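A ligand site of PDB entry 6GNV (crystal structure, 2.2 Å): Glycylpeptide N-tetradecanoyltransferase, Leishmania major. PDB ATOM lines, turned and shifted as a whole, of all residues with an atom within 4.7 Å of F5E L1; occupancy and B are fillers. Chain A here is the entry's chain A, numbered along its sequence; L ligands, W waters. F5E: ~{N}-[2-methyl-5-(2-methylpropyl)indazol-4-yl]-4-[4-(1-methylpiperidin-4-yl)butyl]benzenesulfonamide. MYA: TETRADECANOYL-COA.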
ATOM      1  N   TYR A  70     -23.019  -3.948   0.791  1.00  0.00           N
ATOM      2  CA  TYR A  70     -22.637  -3.437   2.099  1.00  0.00           C
ATOM      3  C   TYR A  70     -22.869  -1.941   2.156  1.00  0.00           C
ATOM      4  O   TYR A  70     -23.648  -1.396   1.385  1.00  0.00           O
ATOM      5  CB  TYR A  70     -21.201  -3.905   2.490  1.00  0.00           C
ATOM      6  CG  TYR A  70     -20.867  -3.811   3.996  1.00  0.00           C
ATOM      7  CD1 TYR A  70     -21.688  -4.395   4.970  1.00  0.00           C
ATOM      8  CD2 TYR A  70     -19.707  -3.136   4.445  1.00  0.00           C
ATOM      9  CE1 TYR A  70     -21.417  -4.272   6.329  1.00  0.00           C
ATOM     10  CE2 TYR A  70     -19.427  -3.018   5.807  1.00  0.00           C
ATOM     11  CZ  TYR A  70     -20.290  -3.593   6.747  1.00  0.00           C
ATOM     12  OH  TYR A  70     -19.998  -3.491   8.083  1.00  0.00           O
ATOM     13  N   VAL A  71     -22.191  -1.268   3.077  1.00  0.00           N
ATOM     14  CA  VAL A  71     -22.505   0.113   3.460  1.00  0.00           C
ATOM     15  C   VAL A  71     -22.238   1.174   2.384  1.00  0.00           C
ATOM     16  O   VAL A  71     -21.194   1.187   1.755  1.00  0.00           O
ATOM     17  CB  VAL A  71     -21.751   0.544   4.748  1.00  0.00           C
ATOM     18  CG1 VAL A  71     -22.129   1.953   5.089  1.00  0.00           C
ATOM     19  CG2 VAL A  71     -22.071  -0.362   5.915  1.00  0.00           C
ATOM     20  N   GLU A  72     -23.265   2.018   2.196  1.00  0.00           N
ATOM     21  CA  GLU A  72     -23.252   3.217   1.376  1.00  0.00           C
ATOM     22  C   GLU A  72     -23.415   4.421   2.264  1.00  0.00           C
ATOM     23  O   GLU A  72     -23.947   4.322   3.362  1.00  0.00           O
ATOM     24  CB  GLU A  72     -24.386   3.154   0.406  1.00  0.00           C
ATOM     25  CG  GLU A  72     -24.250   1.918  -0.476  1.00  0.00           C
ATOM     26  CD  GLU A  72     -25.373   1.773  -1.485  1.00  0.00           C
ATOM     27  OE1 GLU A  72     -25.575   0.679  -2.030  1.00  0.00           O
ATOM     28  OE2 GLU A  72     -26.029   2.758  -1.733  1.00  0.00           O
ATOM     29  N   ASP A  73     -22.914   5.554   1.810  1.00  0.00           N
ATOM     30  CA  ASP A  73     -23.213   6.807   2.486  1.00  0.00           C
ATOM     31  C   ASP A  73     -24.704   7.158   2.241  1.00  0.00           C
ATOM     32  O   ASP A  73     -25.399   6.471   1.453  1.00  0.00           O
ATOM     33  CB  ASP A  73     -22.247   7.918   2.019  1.00  0.00           C
ATOM     34  CG  ASP A  73     -22.392   8.254   0.522  1.00  0.00           C
ATOM     35  OD1 ASP A  73     -22.587   7.354  -0.329  1.00  0.00           O
ATOM     36  OD2 ASP A  73     -22.316   9.459   0.200  1.00  0.00           O
ATOM     37  N   PHE A  78     -21.032   6.268  -2.630  1.00  0.00           N
ATOM     38  CA  PHE A  78     -19.915   5.340  -2.312  1.00  0.00           C
ATOM     39  C   PHE A  78     -20.405   4.081  -1.618  1.00  0.00           C
ATOM     40  O   PHE A  78     -21.267   4.152  -0.740  1.00  0.00           O
ATOM     41  CB  PHE A  78     -18.904   6.039  -1.394  1.00  0.00           C
ATOM     42  CG  PHE A  78     -18.332   7.327  -1.954  1.00  0.00           C
ATOM     43  CD1 PHE A  78     -17.456   7.315  -3.066  1.00  0.00           C
ATOM     44  CD2 PHE A  78     -18.644   8.564  -1.363  1.00  0.00           C
ATOM     45  CE1 PHE A  78     -16.934   8.504  -3.574  1.00  0.00           C
ATOM     46  CE2 PHE A  78     -18.105   9.768  -1.868  1.00  0.00           C
ATOM     47  CZ  PHE A  78     -17.246   9.731  -2.961  1.00  0.00           C
ATOM     48  N   ARG A  79     -19.844   2.930  -1.951  1.00  0.00           N
ATOM     49  CA  ARG A  79     -20.088   1.748  -1.135  1.00  0.00           C
ATOM     50  C   ARG A  79     -18.728   1.138  -0.810  1.00  0.00           C
ATOM     51  O   ARG A  79     -17.848   1.092  -1.677  1.00  0.00           O
ATOM     52  CB  ARG A  79     -20.980   0.744  -1.865  1.00  0.00           C
ATOM     53  CG  ARG A  79     -21.272  -0.549  -1.121  1.00  0.00           C
ATOM     54  CD  ARG A  79     -21.944  -1.630  -1.988  1.00  0.00           C
ATOM     55  NE  ARG A  79     -22.955  -1.014  -2.760  1.00  0.00           N
ATOM     56  CZ  ARG A  79     -23.044  -0.910  -4.086  1.00  0.00           C
ATOM     57  NH1 ARG A  79     -22.270  -1.544  -4.938  1.00  0.00           N
ATOM     58  NH2 ARG A  79     -24.033  -0.171  -4.522  1.00  0.00           N
ATOM     59  N   PHE A  80     -18.545   0.708   0.448  1.00  0.00           N
ATOM     60  CA  PHE A  80     -17.321  -0.016   0.854  1.00  0.00           C
ATOM     61  C   PHE A  80     -17.022  -1.194  -0.062  1.00  0.00           C
ATOM     62  O   PHE A  80     -17.918  -1.987  -0.464  1.00  0.00           O
ATOM     63  CB  PHE A  80     -17.420  -0.517   2.314  1.00  0.00           C
ATOM     64  CG  PHE A  80     -17.356   0.585   3.342  1.00  0.00           C
ATOM     65  CD1 PHE A  80     -16.628   1.738   3.127  1.00  0.00           C
ATOM     66  CD2 PHE A  80     -18.054   0.474   4.510  1.00  0.00           C
ATOM     67  CE1 PHE A  80     -16.583   2.739   4.047  1.00  0.00           C
ATOM     68  CE2 PHE A  80     -17.992   1.489   5.465  1.00  0.00           C
ATOM     69  CZ  PHE A  80     -17.243   2.621   5.227  1.00  0.00           C
ATOM     70  N   ASN A 157     -19.469  -7.160  13.382  1.00  0.00           N
ATOM     71  CA  ASN A 157     -19.175  -6.373  12.201  1.00  0.00           C
ATOM     72  C   ASN A 157     -19.772  -7.073  10.972  1.00  0.00           C
ATOM     73  O   ASN A 157     -20.172  -8.252  11.032  1.00  0.00           O
ATOM     74  CB  ASN A 157     -17.663  -6.219  12.105  1.00  0.00           C
ATOM     75  CG  ASN A 157     -17.203  -4.948  11.380  1.00  0.00           C
ATOM     76  OD1 ASN A 157     -17.921  -4.287  10.685  1.00  0.00           O
ATOM     77  ND2 ASN A 157     -15.934  -4.640  11.562  1.00  0.00           N
ATOM     78  N   THR A 193     -20.590  -0.963  16.217  1.00  0.00           N
ATOM     79  CA  THR A 193     -20.821   0.379  15.729  1.00  0.00           C
ATOM     80  C   THR A 193     -21.692   0.329  14.475  1.00  0.00           C
ATOM     81  O   THR A 193     -21.772  -0.711  13.779  1.00  0.00           O
ATOM     82  CB  THR A 193     -19.509   1.072  15.381  1.00  0.00           C
ATOM     83  OG1 THR A 193     -18.831   0.327  14.359  1.00  0.00           O
ATOM     84  CG2 THR A 193     -18.581   1.260  16.613  1.00  0.00           C
ATOM     85  N   ALA A 194     -22.340   1.441  14.170  1.00  0.00           N
ATOM     86  CA  ALA A 194     -23.169   1.581  12.977  1.00  0.00           C
ATOM     87  C   ALA A 194     -23.256   3.022  12.600  1.00  0.00           C
ATOM     88  O   ALA A 194     -23.057   3.899  13.475  1.00  0.00           O
ATOM     89  CB  ALA A 194     -24.558   1.031  13.201  1.00  0.00           C
ATOM     90  N   GLY A 195     -23.519   3.247  11.304  1.00  0.00           N
ATOM     91  CA  GLY A 195     -23.765   4.573  10.771  1.00  0.00           C
ATOM     92  C   GLY A 195     -25.171   5.062  11.098  1.00  0.00           C
ATOM     93  O   GLY A 195     -25.475   6.239  10.914  1.00  0.00           O
ATOM     94  N   TYR A 207     -17.370  11.558  11.256  1.00  0.00           N
ATOM     95  CA  TYR A 207     -16.244  11.237  10.421  1.00  0.00           C
ATOM     96  C   TYR A 207     -15.578  12.515   9.911  1.00  0.00           C
ATOM     97  O   TYR A 207     -16.232  13.554   9.761  1.00  0.00           O
ATOM     98  CB  TYR A 207     -16.693  10.417   9.207  1.00  0.00           C
ATOM     99  CG  TYR A 207     -16.828   8.921   9.455  1.00  0.00           C
ATOM    100  CD1 TYR A 207     -18.018   8.360   9.925  1.00  0.00           C
ATOM    101  CD2 TYR A 207     -15.794   8.051   9.146  1.00  0.00           C
ATOM    102  CE1 TYR A 207     -18.154   6.997  10.114  1.00  0.00           C
ATOM    103  CE2 TYR A 207     -15.918   6.682   9.328  1.00  0.00           C
ATOM    104  CZ  TYR A 207     -17.103   6.173   9.814  1.00  0.00           C
ATOM    105  OH  TYR A 207     -17.246   4.824  10.010  1.00  0.00           O
ATOM    106  N   HIS A 209     -12.385  13.608   6.943  1.00  0.00           N
ATOM    107  CA  HIS A 209     -11.546  13.164   5.844  1.00  0.00           C
ATOM    108  C   HIS A 209     -10.584  14.255   5.462  1.00  0.00           C
ATOM    109  O   HIS A 209     -10.876  15.406   5.682  1.00  0.00           O
ATOM    110  CB  HIS A 209     -12.391  12.861   4.619  1.00  0.00           C
ATOM    111  CG  HIS A 209     -13.310  13.963   4.219  1.00  0.00           C
ATOM    112  ND1 HIS A 209     -14.632  13.987   4.597  1.00  0.00           N
ATOM    113  CD2 HIS A 209     -13.094  15.093   3.486  1.00  0.00           C
ATOM    114  CE1 HIS A 209     -15.204  15.065   4.089  1.00  0.00           C
ATOM    115  NE2 HIS A 209     -14.290  15.761   3.430  1.00  0.00           N
ATOM    116  N   LEU A 217     -10.811  13.533  -6.327  1.00  0.00           N
ATOM    117  CA  LEU A 217     -11.945  13.693  -5.411  1.00  0.00           C
ATOM    118  C   LEU A 217     -12.968  14.655  -5.959  1.00  0.00           C
ATOM    119  O   LEU A 217     -14.168  14.526  -5.704  1.00  0.00           O
ATOM    120  CB  LEU A 217     -11.481  14.222  -4.050  1.00  0.00           C
ATOM    121  CG  LEU A 217     -10.950  13.218  -3.018  1.00  0.00           C
ATOM    122  CD1 LEU A 217     -10.492  13.980  -1.804  1.00  0.00           C
ATOM    123  CD2 LEU A 217     -12.003  12.201  -2.609  1.00  0.00           C
ATOM    124  N   ARG A 221     -16.871  13.798  -6.371  1.00  0.00           N
ATOM    125  CA  ARG A 221     -17.955  14.187  -5.470  1.00  0.00           C
ATOM    126  C   ARG A 221     -18.797  15.408  -5.801  1.00  0.00           C
ATOM    127  O   ARG A 221     -19.648  15.781  -5.000  1.00  0.00           O
ATOM    128  CB  ARG A 221     -17.397  14.476  -4.094  1.00  0.00           C
ATOM    129  CG  ARG A 221     -16.559  13.389  -3.468  1.00  0.00           C
ATOM    130  CD  ARG A 221     -15.817  14.001  -2.311  1.00  0.00           C
ATOM    131  NE  ARG A 221     -16.750  14.685  -1.427  1.00  0.00           N
ATOM    132  CZ  ARG A 221     -16.430  15.672  -0.594  1.00  0.00           C
ATOM    133  NH1 ARG A 221     -15.175  16.106  -0.506  1.00  0.00           N
ATOM    134  NH2 ARG A 221     -17.372  16.206   0.150  1.00  0.00           N
ATOM    135  N   SER A 320     -13.589   2.326  -1.746  1.00  0.00           N
ATOM    136  CA  SER A 320     -15.055   2.370  -1.965  1.00  0.00           C
ATOM    137  C   SER A 320     -15.318   2.496  -3.458  1.00  0.00           C
ATOM    138  O   SER A 320     -14.641   3.276  -4.153  1.00  0.00           O
ATOM    139  CB  SER A 320     -15.715   3.556  -1.225  1.00  0.00           C
ATOM    140  OG  SER A 320     -15.828   3.368   0.180  1.00  0.00           O
ATOM    141  N   LEU A 331     -12.530   4.826  -5.087  1.00  0.00           N
ATOM    142  CA  LEU A 331     -11.822   5.770  -4.234  1.00  0.00           C
ATOM    143  C   LEU A 331     -10.941   4.983  -3.236  1.00  0.00           C
ATOM    144  O   LEU A 331     -11.420   4.125  -2.518  1.00  0.00           O
ATOM    145  CB  LEU A 331     -12.858   6.653  -3.529  1.00  0.00           C
ATOM    146  CG  LEU A 331     -12.296   7.718  -2.629  1.00  0.00           C
ATOM    147  CD1 LEU A 331     -11.538   8.725  -3.466  1.00  0.00           C
ATOM    148  CD2 LEU A 331     -13.412   8.374  -1.854  1.00  0.00           C
ATOM    149  N   TYR A 335      -7.604   4.655   6.349  1.00  0.00           N
ATOM    150  CA  TYR A 335      -8.327   4.949   7.584  1.00  0.00           C
ATOM    151  C   TYR A 335      -7.357   4.954   8.757  1.00  0.00           C
ATOM    152  O   TYR A 335      -6.603   4.014   8.943  1.00  0.00           O
ATOM    153  CB  TYR A 335      -9.431   3.866   7.852  1.00  0.00           C
ATOM    154  CG  TYR A 335     -10.597   4.048   6.967  1.00  0.00           C
ATOM    155  CD1 TYR A 335     -10.509   3.776   5.603  1.00  0.00           C
ATOM    156  CD2 TYR A 335     -11.750   4.600   7.440  1.00  0.00           C
ATOM    157  CE1 TYR A 335     -11.573   4.032   4.747  1.00  0.00           C
ATOM    158  CE2 TYR A 335     -12.812   4.866   6.594  1.00  0.00           C
ATOM    159  CZ  TYR A 335     -12.728   4.585   5.230  1.00  0.00           C
ATOM    160  OH  TYR A 335     -13.825   4.834   4.398  1.00  0.00           O
ATOM    161  N   VAL A 364      -7.417   9.775  -0.159  1.00  0.00           N
ATOM    162  CA  VAL A 364      -8.088  10.397   0.986  1.00  0.00           C
ATOM    163  C   VAL A 364      -7.766   9.619   2.223  1.00  0.00           C
ATOM    164  O   VAL A 364      -7.500   8.414   2.180  1.00  0.00           O
ATOM    165  CB  VAL A 364      -9.633  10.509   0.819  1.00  0.00           C
ATOM    166  CG1 VAL A 364     -10.341   9.160   0.887  1.00  0.00           C
ATOM    167  CG2 VAL A 364     -10.229  11.469   1.847  1.00  0.00           C
ATOM    168  N   ASN A 366      -9.421   9.010   5.960  1.00  0.00           N
ATOM    169  CA  ASN A 366     -10.642   9.121   6.764  1.00  0.00           C
ATOM    170  C   ASN A 366     -10.431   8.679   8.199  1.00  0.00           C
ATOM    171  O   ASN A 366      -9.528   7.901   8.500  1.00  0.00           O
ATOM    172  CB  ASN A 366     -11.737   8.241   6.192  1.00  0.00           C
ATOM    173  CG  ASN A 366     -12.456   8.869   5.050  1.00  0.00           C
ATOM    174  OD1 ASN A 366     -11.937   9.752   4.382  1.00  0.00           O
ATOM    175  ND2 ASN A 366     -13.713   8.391   4.810  1.00  0.00           N
ATOM    176  N   GLY A 385     -17.092  14.845   7.406  1.00  0.00           N
ATOM    177  CA  GLY A 385     -17.908  14.234   6.365  1.00  0.00           C
ATOM    178  C   GLY A 385     -19.364  14.241   6.813  1.00  0.00           C
ATOM    179  O   GLY A 385     -19.729  14.857   7.824  1.00  0.00           O
ATOM    180  N   ASP A 386     -20.214  13.569   6.063  1.00  0.00           N
ATOM    181  CA  ASP A 386     -21.604  13.503   6.455  1.00  0.00           C
ATOM    182  C   ASP A 386     -21.889  12.274   7.297  1.00  0.00           C
ATOM    183  O   ASP A 386     -22.922  12.212   7.893  1.00  0.00           O
ATOM    184  CB  ASP A 386     -22.550  13.651   5.280  1.00  0.00           C
ATOM    185  CG  ASP A 386     -22.498  12.486   4.366  1.00  0.00           C
ATOM    186  OD1 ASP A 386     -22.053  11.377   4.801  1.00  0.00           O
ATOM    187  OD2 ASP A 386     -22.884  12.668   3.208  1.00  0.00           O
ATOM    188  N   GLY A 387     -20.970  11.324   7.426  1.00  0.00           N
ATOM    189  CA  GLY A 387     -21.196  10.200   8.365  1.00  0.00           C
ATOM    190  C   GLY A 387     -21.038  10.472   9.882  1.00  0.00           C
ATOM    191  O   GLY A 387     -20.291  11.365  10.313  1.00  0.00           O
ATOM    192  N   LEU A 389     -20.397   7.824  13.322  1.00  0.00           N
ATOM    193  CA  LEU A 389     -20.249   6.475  13.809  1.00  0.00           C
ATOM    194  C   LEU A 389     -20.784   6.390  15.240  1.00  0.00           C
ATOM    195  O   LEU A 389     -20.265   7.057  16.148  1.00  0.00           O
ATOM    196  CB  LEU A 389     -18.788   6.017  13.735  1.00  0.00           C
ATOM    197  CG  LEU A 389     -18.605   4.511  14.011  1.00  0.00           C
ATOM    198  CD1 LEU A 389     -19.350   3.703  12.974  1.00  0.00           C
ATOM    199  CD2 LEU A 389     -17.165   4.007  14.104  1.00  0.00           C
ATOM    200  N   MET A 410     -12.915   0.424  15.070  1.00  0.00           N
ATOM    201  CA  MET A 410     -13.599  -0.651  14.314  1.00  0.00           C
ATOM    202  C   MET A 410     -13.340  -0.650  12.806  1.00  0.00           C
ATOM    203  O   MET A 410     -13.275   0.394  12.167  1.00  0.00           O
ATOM    204  CB  MET A 410     -15.104  -0.731  14.654  1.00  0.00           C
ATOM    205  CG  MET A 410     -15.260  -1.360  16.041  1.00  0.00           C
ATOM    206  SD  MET A 410     -16.846  -1.985  16.376  1.00  0.00           S
ATOM    207  CE  MET A 410     -16.928  -3.484  15.415  1.00  0.00           C
ATOM    208  N   LEU A 411     -13.104  -1.842  12.293  1.00  0.00           N
ATOM    209  CA  LEU A 411     -12.703  -2.025  10.901  1.00  0.00           C
ATOM    210  C   LEU A 411     -13.913  -1.966   9.914  1.00  0.00           C
ATOM    211  O   LEU A 411     -15.056  -2.439  10.155  1.00  0.00           O
ATOM    212  CB  LEU A 411     -11.976  -3.359  10.784  1.00  0.00           C
ATOM    213  CG  LEU A 411     -10.755  -3.489  11.679  1.00  0.00           C
ATOM    214  CD1 LEU A 411     -10.251  -4.910  11.563  1.00  0.00           C
ATOM    215  CD2 LEU A 411      -9.679  -2.515  11.249  1.00  0.00           C
ATOM    216  OXT LEU A 411     -13.749  -1.428   8.823  1.00  0.00           O
HETATM  217  C1  F5E L   1     -14.293  12.546   1.287  1.00  0.00           C
HETATM  218  C2  F5E L   1     -14.561  11.076   1.013  1.00  0.00           C
HETATM  219  C3  F5E L   1     -15.514  10.998  -0.135  1.00  0.00           C
HETATM  220  C4  F5E L   1     -15.049  10.432   2.278  1.00  0.00           C
HETATM  221  C5  F5E L   1     -15.657   9.049   2.075  1.00  0.00           C
HETATM  222  C6  F5E L   1     -14.836   8.132   1.418  1.00  0.00           C
HETATM  223  C7  F5E L   1     -15.234   6.841   1.158  1.00  0.00           C
HETATM  224  C8  F5E L   1     -16.493   6.476   1.615  1.00  0.00           C
HETATM  225  C9  F5E L   1     -18.502   6.667   2.616  1.00  0.00           C
HETATM  226  C10 F5E L   1     -17.332   7.390   2.318  1.00  0.00           C
HETATM  227  C11 F5E L   1     -16.956   8.746   2.596  1.00  0.00           C
HETATM  228  C12 F5E L   1     -18.578   8.439   5.622  1.00  0.00           C
HETATM  229  O1  F5E L   1     -18.407  10.938   5.748  1.00  0.00           O
HETATM  230  S   F5E L   1     -17.743   9.773   5.194  1.00  0.00           S
HETATM  231  O2  F5E L   1     -16.440   9.803   5.787  1.00  0.00           O
HETATM  232  N3  F5E L   1     -17.586   9.721   3.476  1.00  0.00           N
HETATM  233  N1  F5E L   1     -17.113   5.263   1.501  1.00  0.00           N
HETATM  234  N2  F5E L   1     -18.358   5.428   2.145  1.00  0.00           N
HETATM  235  C28 F5E L   1     -19.246   4.237   2.174  1.00  0.00           C
HETATM  236  C13 F5E L   1     -17.887   7.307   6.046  1.00  0.00           C
HETATM  237  C14 F5E L   1     -18.584   6.163   6.352  1.00  0.00           C
HETATM  238  C15 F5E L   1     -19.972   6.095   6.263  1.00  0.00           C
HETATM  239  C16 F5E L   1     -20.668   7.218   5.808  1.00  0.00           C
HETATM  240  C17 F5E L   1     -19.964   8.370   5.492  1.00  0.00           C
HETATM  241  C18 F5E L   1     -20.681   4.791   6.598  1.00  0.00           C
HETATM  242  C19 F5E L   1     -21.317   4.652   7.986  1.00  0.00           C
HETATM  243  C20 F5E L   1     -20.404   3.806   8.843  1.00  0.00           C
HETATM  244  C21 F5E L   1     -20.642   2.312   8.654  1.00  0.00           C
HETATM  245  C22 F5E L   1     -19.941   1.528   9.747  1.00  0.00           C
HETATM  246  C23 F5E L   1     -20.205   0.079   9.524  1.00  0.00           C
HETATM  247  C24 F5E L   1     -19.505  -0.803  10.556  1.00  0.00           C
HETATM  248  N4  F5E L   1     -18.118  -0.417  10.730  1.00  0.00           N
HETATM  249  C25 F5E L   1     -17.338  -1.259  11.612  1.00  0.00           C
HETATM  250  C26 F5E L   1     -17.561   0.900  10.456  1.00  0.00           C
HETATM  251  C27 F5E L   1     -18.462   1.796   9.627  1.00  0.00           C
HETATM  252  S1  MYA L   2     -23.301  -1.905  10.959  1.00  0.00           S
HETATM  253  C2  MYA L   2     -23.509  -2.067   9.225  1.00  0.00           C
HETATM  254  C3  MYA L   2     -24.795  -2.751   8.763  1.00  0.00           C
HETATM  255  N4  MYA L   2     -24.816  -2.986   7.332  1.00  0.00           N
HETATM  256  C5  MYA L   2     -25.140  -2.240   6.329  1.00  0.00           C
HETATM  257  O5  MYA L   2     -25.483  -1.143   6.457  1.00  0.00           O
HETATM  258  C6  MYA L   2     -25.068  -2.812   4.957  1.00  0.00           C
HETATM  259  C7  MYA L   2     -26.197  -2.307   4.082  1.00  0.00           C
HETATM  260  N8  MYA L   2     -27.469  -2.622   4.675  1.00  0.00           N
HETATM  261  C9  MYA L   2     -27.971  -3.800   4.905  1.00  0.00           C
HETATM  262  O9  MYA L   2     -27.412  -4.753   4.567  1.00  0.00           O
HETATM  263  C10 MYA L   2     -29.331  -3.966   5.548  1.00  0.00           C
HETATM  264  O10 MYA L   2     -30.098  -2.800   5.361  1.00  0.00           O
HETATM  265  C11 MYA L   2     -29.276  -4.350   7.047  1.00  0.00           C
HETATM  266  C12 MYA L   2     -30.651  -4.323   7.651  1.00  0.00           C
HETATM  267  C13 MYA L   2     -28.455  -3.325   7.806  1.00  0.00           C
HETATM  268  C14 MYA L   2     -28.651  -5.726   7.274  1.00  0.00           C
HETATM  269  N1A MYA L   2     -27.710  -2.816  13.048  1.00  0.00           N
HETATM  270  O1A MYA L   2     -33.994  -7.163   7.975  1.00  0.00           O
HETATM  271  P1A MYA L   2     -34.711  -5.953   8.204  1.00  0.00           P
HETATM  272  C1X MYA L   2     -32.650  -3.077  12.319  1.00  0.00           C
HETATM  273  C2A MYA L   2     -28.643  -3.371  13.747  1.00  0.00           C
HETATM  274  O2A MYA L   2     -36.048  -5.924   7.719  1.00  0.00           O
HETATM  275  P2A MYA L   2     -32.880  -4.783   6.444  1.00  0.00           P
HETATM  276  C2M MYA L   2     -22.865  -3.404  11.514  1.00  0.00           C
HETATM  277  O2M MYA L   2     -22.410  -4.212  10.794  1.00  0.00           O
HETATM  278  C2X MYA L   2     -33.860  -2.184  12.230  1.00  0.00           C
HETATM  279  O2X MYA L   2     -33.854  -1.132  13.165  1.00  0.00           O
HETATM  280  N3A MYA L   2     -29.895  -3.314  13.387  1.00  0.00           N
HETATM  281  O3A MYA L   2     -34.008  -4.735   7.534  1.00  0.00           O
HETATM  282  C3M MYA L   2     -23.056  -3.775  12.974  1.00  0.00           C
HETATM  283  C3X MYA L   2     -35.006  -3.170  12.380  1.00  0.00           C
HETATM  284  O3X MYA L   2     -35.389  -3.467  13.692  1.00  0.00           O
HETATM  285  P3X MYA L   2     -36.527  -2.736  14.429  1.00  0.00           P
HETATM  286  C4A MYA L   2     -30.247  -2.698  12.298  1.00  0.00           C
HETATM  287  O4A MYA L   2     -32.761  -3.456   6.056  1.00  0.00           O
HETATM  288  C4M MYA L   2     -24.301  -4.597  13.190  1.00  0.00           C
HETATM  289  C4X MYA L   2     -34.459  -4.404  11.740  1.00  0.00           C
HETATM  290  O4X MYA L   2     -33.054  -4.245  11.696  1.00  0.00           O
HETATM  291  C5A MYA L   2     -29.308  -2.101  11.533  1.00  0.00           C
HETATM  292  O5A MYA L   2     -33.160  -5.701   5.415  1.00  0.00           O
HETATM  293  C5M MYA L   2     -24.691  -4.847  14.619  1.00  0.00           C
HETATM  294  C5X MYA L   2     -35.061  -4.531  10.372  1.00  0.00           C
HETATM  295  O5X MYA L   2     -34.622  -5.672   9.700  1.00  0.00           O
HETATM  296  C6A MYA L   2     -27.989  -2.166  11.955  1.00  0.00           C
HETATM  297  N6A MYA L   2     -26.977  -1.624  11.312  1.00  0.00           N
HETATM  298  O6A MYA L   2     -31.578  -5.257   7.154  1.00  0.00           O
HETATM  299  C6M MYA L   2     -25.965  -5.667  14.690  1.00  0.00           C
HETATM  300  N7A MYA L   2     -29.961  -1.602  10.532  1.00  0.00           N
HETATM  301  O7A MYA L   2     -36.356  -1.256  14.696  1.00  0.00           O
HETATM  302  C7M MYA L   2     -26.467  -5.877  16.094  1.00  0.00           C
HETATM  303  C8A MYA L   2     -31.222  -1.847  10.679  1.00  0.00           C
HETATM  304  O8A MYA L   2     -37.880  -3.127  13.910  1.00  0.00           O
HETATM  305  C8M MYA L   2     -25.594  -6.826  16.901  1.00  0.00           C
HETATM  306  N9A MYA L   2     -31.401  -2.543  11.744  1.00  0.00           N
HETATM  307  O9A MYA L   2     -36.430  -3.007  15.915  1.00  0.00           O
HETATM  308  C9M MYA L   2     -26.050  -6.992  18.332  1.00  0.00           C
HETATM  309  CAM MYA L   2     -25.097  -7.801  19.186  1.00  0.00           C
HETATM  310  CBM MYA L   2     -25.161  -9.264  18.864  1.00  0.00           C
HETATM  311  CCM MYA L   2     -24.213 -10.071  19.705  1.00  0.00           C
HETATM  312  CDM MYA L   2     -24.680 -10.374  21.120  1.00  0.00           C
HETATM  313  CEM MYA L   2     -23.750 -11.360  21.812  1.00  0.00           C
HETATM  314  CFM MYA L   2     -23.848 -11.411  23.319  1.00  0.00           C
HETATM  315  O   HOH W   1     -17.643  -2.563   8.690  1.00  0.00           O
HETATM  316  O   HOH W   2     -20.433  10.656   2.419  1.00  0.00           O
HETATM  317  O   HOH W   3     -15.199  11.976   6.151  1.00  0.00           O
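The side-chain hydroxyl (OG) of Ser 320 lies within hydrogen-bond range of a nitrogen (N1) of F5E L1 (2.6 Å). The chain-end carboxylate (O) of Leu 411 lies within salt-bridge range of a nitrogen (N4) of F5E L1 (3.7 Å). O1 of F5E L1 is in hydrogen-bond range of N of Gly 387, 3.1 Å away. The backbone NH (N) of Asp 386 lies within hydrogen-bond range of an oxygen (O1) of F5E L1 (3.2 Å). O2 of F5E L1 sits at hydrogen-bond distance from ND2 of Asn 366, 3.2 Å away.
N of Leu 331 sits at hydrogen-bond distance from O of Ser 320. The chain-end carboxylate (O) of Leu 411 is in hydrogen-bond range of the side-chain amide nitrogen (ND2) of Asn 157 (2.8 Å). The backbone carbonyl oxygen (O) of Gly 387 is in hydrogen-bond range of the backbone NH (N) of Tyr 207. The side-chain amide oxygen (OD1) of Asn 157 is in hydrogen-bond range of the side-chain hydroxyl (OH) of Tyr 70 (3.4 Å). N of Gly 385 is in hydrogen-bond range of O of Tyr 207, 2.8 Å away. N of Phe 78 lies within hydrogen-bond range of OD1 of Asp 73 (3.0 Å). OG1 of Thr 193 sits at hydrogen-bond distance from SD of Met 410 (3.7 Å). The backbone NH of Phe 80 sits at hydrogen-bond distance from the backbone carbonyl oxygen of Val 71 (3.0 Å).
Tyr 70 touches F5E L1. CG1 of Val 71 touches C18 of F5E L1, 3.5 Å away. Asp 73 touches F5E L1. Phe 78 touches F5E L1. CE1 of Phe 80 touches C28 of F5E L1, at 3.6 Å. Asn 157 touches F5E L1. OG1 of Thr 193 touches C25 of F5E L1, at 3.5 Å. Gly 195 touches F5E L1. Tyr 207 touches F5E L1. His 209 touches F5E L1 (CG to C1, 3.4 Å). CD of Arg 221 touches C3 of F5E L1 (3.7 Å). Leu 331 touches F5E L1. Gly 385 touches F5E L1. Leu 389 touches F5E L1 (CD1 to C22, 3.9 Å). Met 410 touches F5E L1. Hydrophobic or aromatic side chains within 4 Å of F5E L1: Val 71, Phe 78, Phe 80, Tyr 207, His 209, Leu 331, Leu 389 and Met 410. Within 4 Å of F5E L1: Tyr 70, Val 71, Asp 73, Phe 78, Phe 80, Asn 157, Thr 193, Gly 195, Tyr 207, His 209, Arg 221, Ser 320, Leu 331, Asn 366, Gly 385, Asp 386, Gly 387, Leu 389, Met 410 and Leu 411. The nearest printed residue that does not touch F5E L1 is Tyr 335 (4.1 Å).
Water W3 bridges O2 of F5E L1 (2.5 Å) and ND1 of His 209 (2.6 Å). Water W1 lies within hydrogen-bond range of OH of Tyr 70 (2.6 Å), OD1 of Asn 157 (2.7 Å) and O of Leu 411 (3.0 Å). Water W2 lies within hydrogen-bond range of the side-chain carboxylate (OD1) of Asp 386 (3.0 Å), the side-chain carboxylate (OD2) of Asp 73 (3.1 Å) and a nitrogen (N3) of F5E L1 (3.2 Å).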
